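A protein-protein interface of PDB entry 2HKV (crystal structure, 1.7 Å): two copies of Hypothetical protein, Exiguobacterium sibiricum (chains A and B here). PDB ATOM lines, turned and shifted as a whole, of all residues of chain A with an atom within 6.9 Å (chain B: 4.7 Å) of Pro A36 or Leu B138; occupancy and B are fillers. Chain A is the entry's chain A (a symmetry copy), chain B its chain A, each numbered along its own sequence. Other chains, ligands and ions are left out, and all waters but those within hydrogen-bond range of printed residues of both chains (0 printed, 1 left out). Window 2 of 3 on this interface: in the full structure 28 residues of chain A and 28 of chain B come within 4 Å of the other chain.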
ATOM      1  N   ASP A  31      10.329   8.535  20.944  1.00  0.00           N
ATOM      2  CA  ASP A  31      11.539   8.792  21.735  1.00  0.00           C
ATOM      3  C   ASP A  31      12.419   7.574  22.053  1.00  0.00           C
ATOM      4  O   ASP A  31      13.534   7.727  22.594  1.00  0.00           O
ATOM      5  CB  ASP A  31      11.134   9.492  23.047  1.00  0.00           C
ATOM      6  CG  ASP A  31      10.639  10.925  22.809  1.00  0.00           C
ATOM      7  OD1 ASP A  31      11.062  11.559  21.803  1.00  0.00           O
ATOM      8  OD2 ASP A  31       9.849  11.425  23.631  1.00  0.00           O
ATOM      9  N   ASP A  33      14.248   5.419  20.390  1.00  0.00           N
ATOM     10  CA  ASP A  33      15.605   5.310  19.847  1.00  0.00           C
ATOM     11  C   ASP A  33      16.477   6.541  20.037  1.00  0.00           C
ATOM     12  O   ASP A  33      17.635   6.551  19.602  1.00  0.00           O
ATOM     13  CB  ASP A  33      15.553   4.965  18.343  1.00  0.00           C
ATOM     14  CG  ASP A  33      15.081   3.547  18.110  1.00  0.00           C
ATOM     15  OD1 ASP A  33      15.561   2.645  18.856  1.00  0.00           O
ATOM     16  OD2 ASP A  33      14.215   3.342  17.224  1.00  0.00           O
ATOM     17  N   LYS A  34      15.926   7.581  20.644  1.00  0.00           N
ATOM     18  CA  LYS A  34      16.696   8.777  20.940  1.00  0.00           C
ATOM     19  C   LYS A  34      17.847   8.455  21.916  1.00  0.00           C
ATOM     20  O   LYS A  34      17.704   7.631  22.852  1.00  0.00           O
ATOM     21  CB  LYS A  34      15.785   9.888  21.511  1.00  0.00           C
ATOM     22  CG  LYS A  34      14.850  10.551  20.488  1.00  0.00           C
ATOM     23  CD  LYS A  34      14.992  12.107  20.533  1.00  0.00           C
ATOM     24  CE  LYS A  34      13.987  12.898  19.643  1.00  0.00           C
ATOM     25  NZ  LYS A  34      12.613  12.270  19.369  1.00  0.00           N
ATOM     26  N   ARG A  35      18.984   9.108  21.682  1.00  0.00           N
ATOM     27  CA  ARG A  35      20.160   9.021  22.567  1.00  0.00           C
ATOM     28  C   ARG A  35      20.532  10.428  22.997  1.00  0.00           C
ATOM     29  O   ARG A  35      21.339  11.074  22.334  1.00  0.00           O
ATOM     30  CB  ARG A  35      21.369   8.393  21.837  1.00  0.00           C
ATOM     31  CG  ARG A  35      21.048   7.050  21.217  1.00  0.00           C
ATOM     32  CD  ARG A  35      22.251   6.432  20.449  1.00  0.00           C
ATOM     33  NE  ARG A  35      22.254   4.978  20.629  1.00  0.00           N
ATOM     34  CZ  ARG A  35      21.395   4.142  20.039  1.00  0.00           C
ATOM     35  NH1 ARG A  35      20.443   4.591  19.208  1.00  0.00           N
ATOM     36  NH2 ARG A  35      21.474   2.835  20.294  1.00  0.00           N
ATOM     37  N   PRO A  36      19.925  10.922  24.085  1.00  0.00           N
ATOM     38  CA  PRO A  36      20.158  12.283  24.552  1.00  0.00           C
ATOM     39  C   PRO A  36      21.610  12.541  24.981  1.00  0.00           C
ATOM     40  O   PRO A  36      22.022  13.677  24.991  1.00  0.00           O
ATOM     41  CB  PRO A  36      19.216  12.409  25.773  1.00  0.00           C
ATOM     42  CG  PRO A  36      18.246  11.282  25.667  1.00  0.00           C
ATOM     43  CD  PRO A  36      18.974  10.193  24.941  1.00  0.00           C
ATOM     44  N   ILE A  37      22.345  11.515  25.395  1.00  0.00           N
ATOM     45  CA  ILE A  37      23.769  11.652  25.711  1.00  0.00           C
ATOM     46  C   ILE A  37      24.586  10.860  24.686  1.00  0.00           C
ATOM     47  O   ILE A  37      24.667   9.636  24.759  1.00  0.00           O
ATOM     48  CB  ILE A  37      24.091  11.122  27.131  1.00  0.00           C
ATOM     49  CG1 ILE A  37      23.105  11.698  28.151  1.00  0.00           C
ATOM     50  CG2 ILE A  37      25.528  11.433  27.513  1.00  0.00           C
ATOM     51  CD1 ILE A  37      23.551  11.539  29.586  1.00  0.00           C
ATOM     52  N   SER A  38      25.177  11.569  23.726  1.00  0.00           N
ATOM     53  CA  SER A  38      25.906  10.926  22.619  1.00  0.00           C
ATOM     54  C   SER A  38      26.971  10.032  23.211  1.00  0.00           C
ATOM     55  O   SER A  38      27.658  10.437  24.140  1.00  0.00           O
ATOM     56  CB  SER A  38      26.520  11.965  21.665  1.00  0.00           C
ATOM     57  OG  SER A  38      27.742  12.483  22.173  1.00  0.00           O
ATOM     58  N   LYS A  40      26.130   7.049  24.673  1.00  0.00           N
ATOM     59  CA  LYS A  40      25.513   6.192  25.667  1.00  0.00           C
ATOM     60  C   LYS A  40      24.245   5.498  25.171  1.00  0.00           C
ATOM     61  O   LYS A  40      23.797   5.749  24.058  1.00  0.00           O
ATOM     62  CB  LYS A  40      25.253   7.011  26.938  1.00  0.00           C
ATOM     63  CG  LYS A  40      26.517   7.697  27.487  1.00  0.00           C
ATOM     64  CD  LYS A  40      27.690   6.699  27.632  1.00  0.00           C
ATOM     65  CE  LYS A  40      28.701   7.096  28.706  1.00  0.00           C
ATOM     66  NZ  LYS A  40      29.988   6.339  28.592  1.00  0.00           N
ATOM     67  N   ARG A  41      23.694   4.620  26.012  1.00  0.00           N
ATOM     68  CA  ARG A  41      22.497   3.843  25.698  1.00  0.00           C
ATOM     69  C   ARG A  41      21.365   4.776  25.212  1.00  0.00           C
ATOM     70  O   ARG A  41      21.255   5.917  25.647  1.00  0.00           O
ATOM     71  CB  ARG A  41      22.034   3.080  26.920  1.00  0.00           C
ATOM     72  CG  ARG A  41      22.625   1.696  27.170  1.00  0.00           C
ATOM     73  CD  ARG A  41      22.325   1.269  28.549  1.00  0.00           C
ATOM     74  NE  ARG A  41      22.496  -0.163  28.751  1.00  0.00           N
ATOM     75  CZ  ARG A  41      23.499  -0.685  29.450  1.00  0.00           C
ATOM     76  NH1 ARG A  41      24.382   0.107  30.044  1.00  0.00           N
ATOM     77  NH2 ARG A  41      23.630  -2.004  29.561  1.00  0.00           N
ATOM     78  N   SER A  42      20.542   4.287  24.301  1.00  0.00           N
ATOM     79  CA  SER A  42      19.309   4.969  23.956  1.00  0.00           C
ATOM     80  C   SER A  42      18.269   4.883  25.109  1.00  0.00           C
ATOM     81  O   SER A  42      18.479   4.156  26.066  1.00  0.00           O
ATOM     82  CB  SER A  42      18.712   4.368  22.691  1.00  0.00           C
ATOM     83  OG  SER A  42      18.169   3.092  22.976  1.00  0.00           O
ATOM     84  N   VAL A  43      17.174   5.662  25.027  1.00  0.00           N
ATOM     85  CA  VAL A  43      16.071   5.580  25.961  1.00  0.00           C
ATOM     86  C   VAL A  43      15.585   4.146  26.089  1.00  0.00           C
ATOM     87  O   VAL A  43      15.407   3.619  27.206  1.00  0.00           O
ATOM     88  CB  VAL A  43      14.865   6.455  25.472  1.00  0.00           C
ATOM     89  CG1 VAL A  43      13.658   6.181  26.277  1.00  0.00           C
ATOM     90  CG2 VAL A  43      15.212   7.907  25.527  1.00  0.00           C
ATOM     91  N   ASP A 134      17.053  11.722  33.760  1.00  0.00           N
ATOM     92  CA  ASP A 134      17.858  12.745  33.070  1.00  0.00           C
ATOM     93  C   ASP A 134      17.572  12.742  31.560  1.00  0.00           C
ATOM     94  O   ASP A 134      17.464  13.802  30.958  1.00  0.00           O
ATOM     95  CB  ASP A 134      19.345  12.530  33.260  1.00  0.00           C
ATOM     96  CG  ASP A 134      19.818  12.830  34.660  1.00  0.00           C
ATOM     97  OD1 ASP A 134      19.072  13.493  35.435  1.00  0.00           O
ATOM     98  OD2 ASP A 134      20.984  12.404  34.963  1.00  0.00           O
ATOM     99  N   TYR A 135      17.445  11.563  30.964  1.00  0.00           N
ATOM    100  CA  TYR A 135      17.145  11.478  29.553  1.00  0.00           C
ATOM    101  C   TYR A 135      15.801  12.140  29.235  1.00  0.00           C
ATOM    102  O   TYR A 135      15.700  12.889  28.261  1.00  0.00           O
ATOM    103  CB  TYR A 135      17.015  10.036  29.095  1.00  0.00           C
ATOM    104  CG  TYR A 135      18.299   9.290  28.817  1.00  0.00           C
ATOM    105  CD1 TYR A 135      19.522   9.743  29.281  1.00  0.00           C
ATOM    106  CD2 TYR A 135      18.268   8.107  28.094  1.00  0.00           C
ATOM    107  CE1 TYR A 135      20.687   9.013  29.060  1.00  0.00           C
ATOM    108  CE2 TYR A 135      19.423   7.397  27.835  1.00  0.00           C
ATOM    109  CZ  TYR A 135      20.631   7.855  28.313  1.00  0.00           C
ATOM    110  OH  TYR A 135      21.773   7.128  28.059  1.00  0.00           O
ATOM    111  N   LEU A 136      14.767  11.790  30.002  1.00  0.00           N
ATOM    112  CA  LEU A 136      13.431  12.305  29.710  1.00  0.00           C
ATOM    113  C   LEU A 136      13.425  13.817  29.925  1.00  0.00           C
ATOM    114  O   LEU A 136      12.896  14.540  29.122  1.00  0.00           O
ATOM    115  CB  LEU A 136      12.350  11.588  30.556  1.00  0.00           C
ATOM    116  CG  LEU A 136      12.122  10.103  30.215  1.00  0.00           C
ATOM    117  CD1 LEU A 136      10.893   9.555  31.018  1.00  0.00           C
ATOM    118  CD2 LEU A 136      12.023   9.758  28.752  1.00  0.00           C
ATOM    119  N   LEU A 138      16.083  15.811  29.607  1.00  0.00           N
ATOM    120  CA  LEU A 138      16.807  16.296  28.407  1.00  0.00           C
ATOM    121  C   LEU A 138      15.873  16.422  27.191  1.00  0.00           C
ATOM    122  O   LEU A 138      16.040  17.299  26.350  1.00  0.00           O
ATOM    123  CB  LEU A 138      17.940  15.359  28.032  1.00  0.00           C
ATOM    124  CG  LEU A 138      19.245  15.545  28.841  1.00  0.00           C
ATOM    125  CD1 LEU A 138      20.214  14.363  28.677  1.00  0.00           C
ATOM    126  CD2 LEU A 138      19.918  16.788  28.463  1.00  0.00           C
ATOM    127  N   LEU A 139      14.859  15.557  27.134  1.00  0.00           N
ATOM    128  CA  LEU A 139      13.906  15.554  26.037  1.00  0.00           C
ATOM    129  C   LEU A 139      12.702  16.472  26.303  1.00  0.00           C
ATOM    130  O   LEU A 139      11.726  16.412  25.586  1.00  0.00           O
ATOM    131  CB  LEU A 139      13.470  14.114  25.730  1.00  0.00           C
ATOM    132  CG  LEU A 139      14.549  13.197  25.119  1.00  0.00           C
ATOM    133  CD1 LEU A 139      14.124  11.696  25.128  1.00  0.00           C
ATOM    134  CD2 LEU A 139      14.924  13.636  23.706  1.00  0.00           C
ATOM    135  N   PRO B  36      23.938  21.415  32.151  1.00  0.00           N
ATOM    136  CA  PRO B  36      23.750  20.591  30.964  1.00  0.00           C
ATOM    137  C   PRO B  36      22.286  20.191  30.724  1.00  0.00           C
ATOM    138  O   PRO B  36      21.942  19.879  29.609  1.00  0.00           O
ATOM    139  CB  PRO B  36      24.598  19.331  31.263  1.00  0.00           C
ATOM    140  CG  PRO B  36      25.505  19.699  32.387  1.00  0.00           C
ATOM    141  CD  PRO B  36      24.774  20.750  33.165  1.00  0.00           C
ATOM    142  N   ILE B  37      21.461  20.134  31.764  1.00  0.00           N
ATOM    143  CA  ILE B  37      20.028  19.876  31.610  1.00  0.00           C
ATOM    144  C   ILE B  37      19.248  21.132  32.013  1.00  0.00           C
ATOM    145  O   ILE B  37      19.091  21.418  33.198  1.00  0.00           O
ATOM    146  CB  ILE B  37      19.563  18.690  32.492  1.00  0.00           C
ATOM    147  CG1 ILE B  37      20.499  17.492  32.308  1.00  0.00           C
ATOM    148  CG2 ILE B  37      18.121  18.319  32.190  1.00  0.00           C
ATOM    149  CD1 ILE B  37      19.932  16.191  32.830  1.00  0.00           C
ATOM    150  N   ASP B 134      26.081  11.767  34.348  1.00  0.00           N
ATOM    151  CA  ASP B 134      25.393  12.179  33.112  1.00  0.00           C
ATOM    152  C   ASP B 134      25.798  13.607  32.710  1.00  0.00           C
ATOM    153  O   ASP B 134      26.014  13.871  31.535  1.00  0.00           O
ATOM    154  CB  ASP B 134      23.886  12.147  33.254  1.00  0.00           C
ATOM    155  CG  ASP B 134      23.322  10.751  33.325  1.00  0.00           C
ATOM    156  OD1 ASP B 134      24.043   9.775  32.970  1.00  0.00           O
ATOM    157  OD2 ASP B 134      22.113  10.651  33.727  1.00  0.00           O
ATOM    158  N   TYR B 135      25.902  14.508  33.679  1.00  0.00           N
ATOM    159  CA  TYR B 135      26.306  15.864  33.385  1.00  0.00           C
ATOM    160  C   TYR B 135      27.707  15.899  32.768  1.00  0.00           C
ATOM    161  O   TYR B 135      27.929  16.608  31.785  1.00  0.00           O
ATOM    162  CB  TYR B 135      26.387  16.709  34.644  1.00  0.00           C
ATOM    163  CG  TYR B 135      25.088  17.264  35.178  1.00  0.00           C
ATOM    164  CD1 TYR B 135      23.861  16.763  34.779  1.00  0.00           C
ATOM    165  CD2 TYR B 135      25.106  18.294  36.106  1.00  0.00           C
ATOM    166  CE1 TYR B 135      22.675  17.252  35.322  1.00  0.00           C
ATOM    167  CE2 TYR B 135      23.935  18.813  36.621  1.00  0.00           C
ATOM    168  CZ  TYR B 135      22.721  18.296  36.223  1.00  0.00           C
ATOM    169  OH  TYR B 135      21.563  18.815  36.756  1.00  0.00           O
ATOM    170  N   LEU B 136      28.655  15.205  33.401  1.00  0.00           N
ATOM    171  CA  LEU B 136      30.038  15.258  32.931  1.00  0.00           C
ATOM    172  C   LEU B 136      30.117  14.617  31.547  1.00  0.00           C
ATOM    173  O   LEU B 136      30.749  15.145  30.671  1.00  0.00           O
ATOM    174  CB  LEU B 136      31.006  14.592  33.942  1.00  0.00           C
ATOM    175  CG  LEU B 136      31.172  15.331  35.282  1.00  0.00           C
ATOM    176  CD1 LEU B 136      32.299  14.649  36.130  1.00  0.00           C
ATOM    177  CD2 LEU B 136      31.366  16.823  35.207  1.00  0.00           C
ATOM    178  N   ASN B 137      29.399  13.520  31.330  1.00  0.00           N
ATOM    179  CA  ASN B 137      29.353  12.912  29.998  1.00  0.00           C
ATOM    180  C   ASN B 137      28.662  13.795  28.951  1.00  0.00           C
ATOM    181  O   ASN B 137      29.099  13.856  27.789  1.00  0.00           O
ATOM    182  CB  ASN B 137      28.679  11.551  30.063  1.00  0.00           C
ATOM    183  CG  ASN B 137      29.603  10.462  30.600  1.00  0.00           C
ATOM    184  OD1 ASN B 137      30.823  10.505  30.406  1.00  0.00           O
ATOM    185  ND2 ASN B 137      29.016   9.498  31.283  1.00  0.00           N
ATOM    186  N   LEU B 138      27.612  14.504  29.342  1.00  0.00           N
ATOM    187  CA  LEU B 138      27.016  15.555  28.481  1.00  0.00           C
ATOM    188  C   LEU B 138      28.049  16.625  28.091  1.00  0.00           C
ATOM    189  O   LEU B 138      28.000  17.187  27.002  1.00  0.00           O
ATOM    190  CB  LEU B 138      25.863  16.249  29.182  1.00  0.00           C
ATOM    191  CG  LEU B 138      24.511  15.498  29.131  1.00  0.00           C
ATOM    192  CD1 LEU B 138      23.490  16.052  30.137  1.00  0.00           C
ATOM    193  CD2 LEU B 138      23.945  15.541  27.782  1.00  0.00           C
ATOM    194  N   LEU B 139      29.012  16.869  28.982  1.00  0.00           N
ATOM    195  CA  LEU B 139      30.046  17.863  28.750  1.00  0.00           C
ATOM    196  C   LEU B 139      31.277  17.273  28.043  1.00  0.00           C
ATOM    197  O   LEU B 139      32.301  17.919  27.973  1.00  0.00           O
ATOM    198  CB  LEU B 139      30.420  18.544  30.074  1.00  0.00           C
ATOM    199  CG  LEU B 139      29.340  19.455  30.693  1.00  0.00           C
ATOM    200  CD1 LEU B 139      29.674  19.854  32.164  1.00  0.00           C
ATOM    201  CD2 LEU B 139      29.105  20.703  29.843  1.00  0.00           C
ATOM    202  N   GLY B 140      31.184  16.045  27.535  1.00  0.00           N
ATOM    203  CA  GLY B 140      32.282  15.457  26.754  1.00  0.00           C
ATOM    204  C   GLY B 140      33.402  14.822  27.549  1.00  0.00           C
ATOM    205  O   GLY B 140      34.447  14.534  27.002  1.00  0.00           O
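The side-chain carboxylate (OD2) of Asp A134 lies close to the side-chain carboxylate (OD2) of Asp B134, 2.4 Å away.
Leu B138 touches Pro A36 (CD2 to O, 3.9 Å).
CD1 of Ile A37 touches CB of Asp B134 (3.7 Å).
Ile A37 touches Leu B138 (CG1 to CD2, 3.95 Å).
ND2 of Asn B137 touches CE of Lys A40, at 3.5 Å.
Asp A134 touches Ile B37.
Leu A138 touches Pro B36.
Ile B37 touches Leu A138.
CD1 of Leu A138 touches CD1 of Leu B138, 3.96 Å away.
Asp A33 touches none of the printed residues of chain B.
Pro A36 touches one residue of chain B.
Of the printed residues of chain B, Ile A37 touches Asp B134 and Leu B138.
Of the printed residues of chain B, Lys A40 touches Asn B137.
Of the printed residues of chain B, Leu A138 touches Pro B36, Ile B37 and Leu B138.
Of the printed residues of chain A, Pro B36 touches Leu A138 (3.9 Å).
Of the printed residues of chain A, Ile B37 touches Asp A134 (3.7 Å) and Leu A138 (3.95 Å).
Leu B138 touches just these residues of chain A: Pro A36, Ile A37 and Leu A138.
Leu B139 touches none of the printed residues of chain A.
The nearest residue of chain A that does not touch Leu B138 is Ser A38 (5.8 Å).
The nearest printed residue of chain B that does not touch Ile A37 is Asn B137 (4.1 Å).
Along chain B the printed residues that touch a printed residue of chain A span positions 36 to 138.
Among the printed residues, 9 pairs touch across the chains.
Among the printed residues, no Asp or Glu carboxylate lies within 4 Å of a Lys or Arg side-chain nitrogen of the other chain.
Pro A36 touches Leu B138, and with the chains exchanged Leu A138 touches Pro B36.
Ile A37 touches Asp B134, and with the chains exchanged Asp A134 touches Ile B37.
Asp A134 touches its own counterpart, Asp B134.
Leu B138 touches its own counterpart, Leu A138.
7 positions are printed for both chains.
Of the 9 pairs that touch across the chains among the printed residues, 8 have their exchanged pair printed and touching as well.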
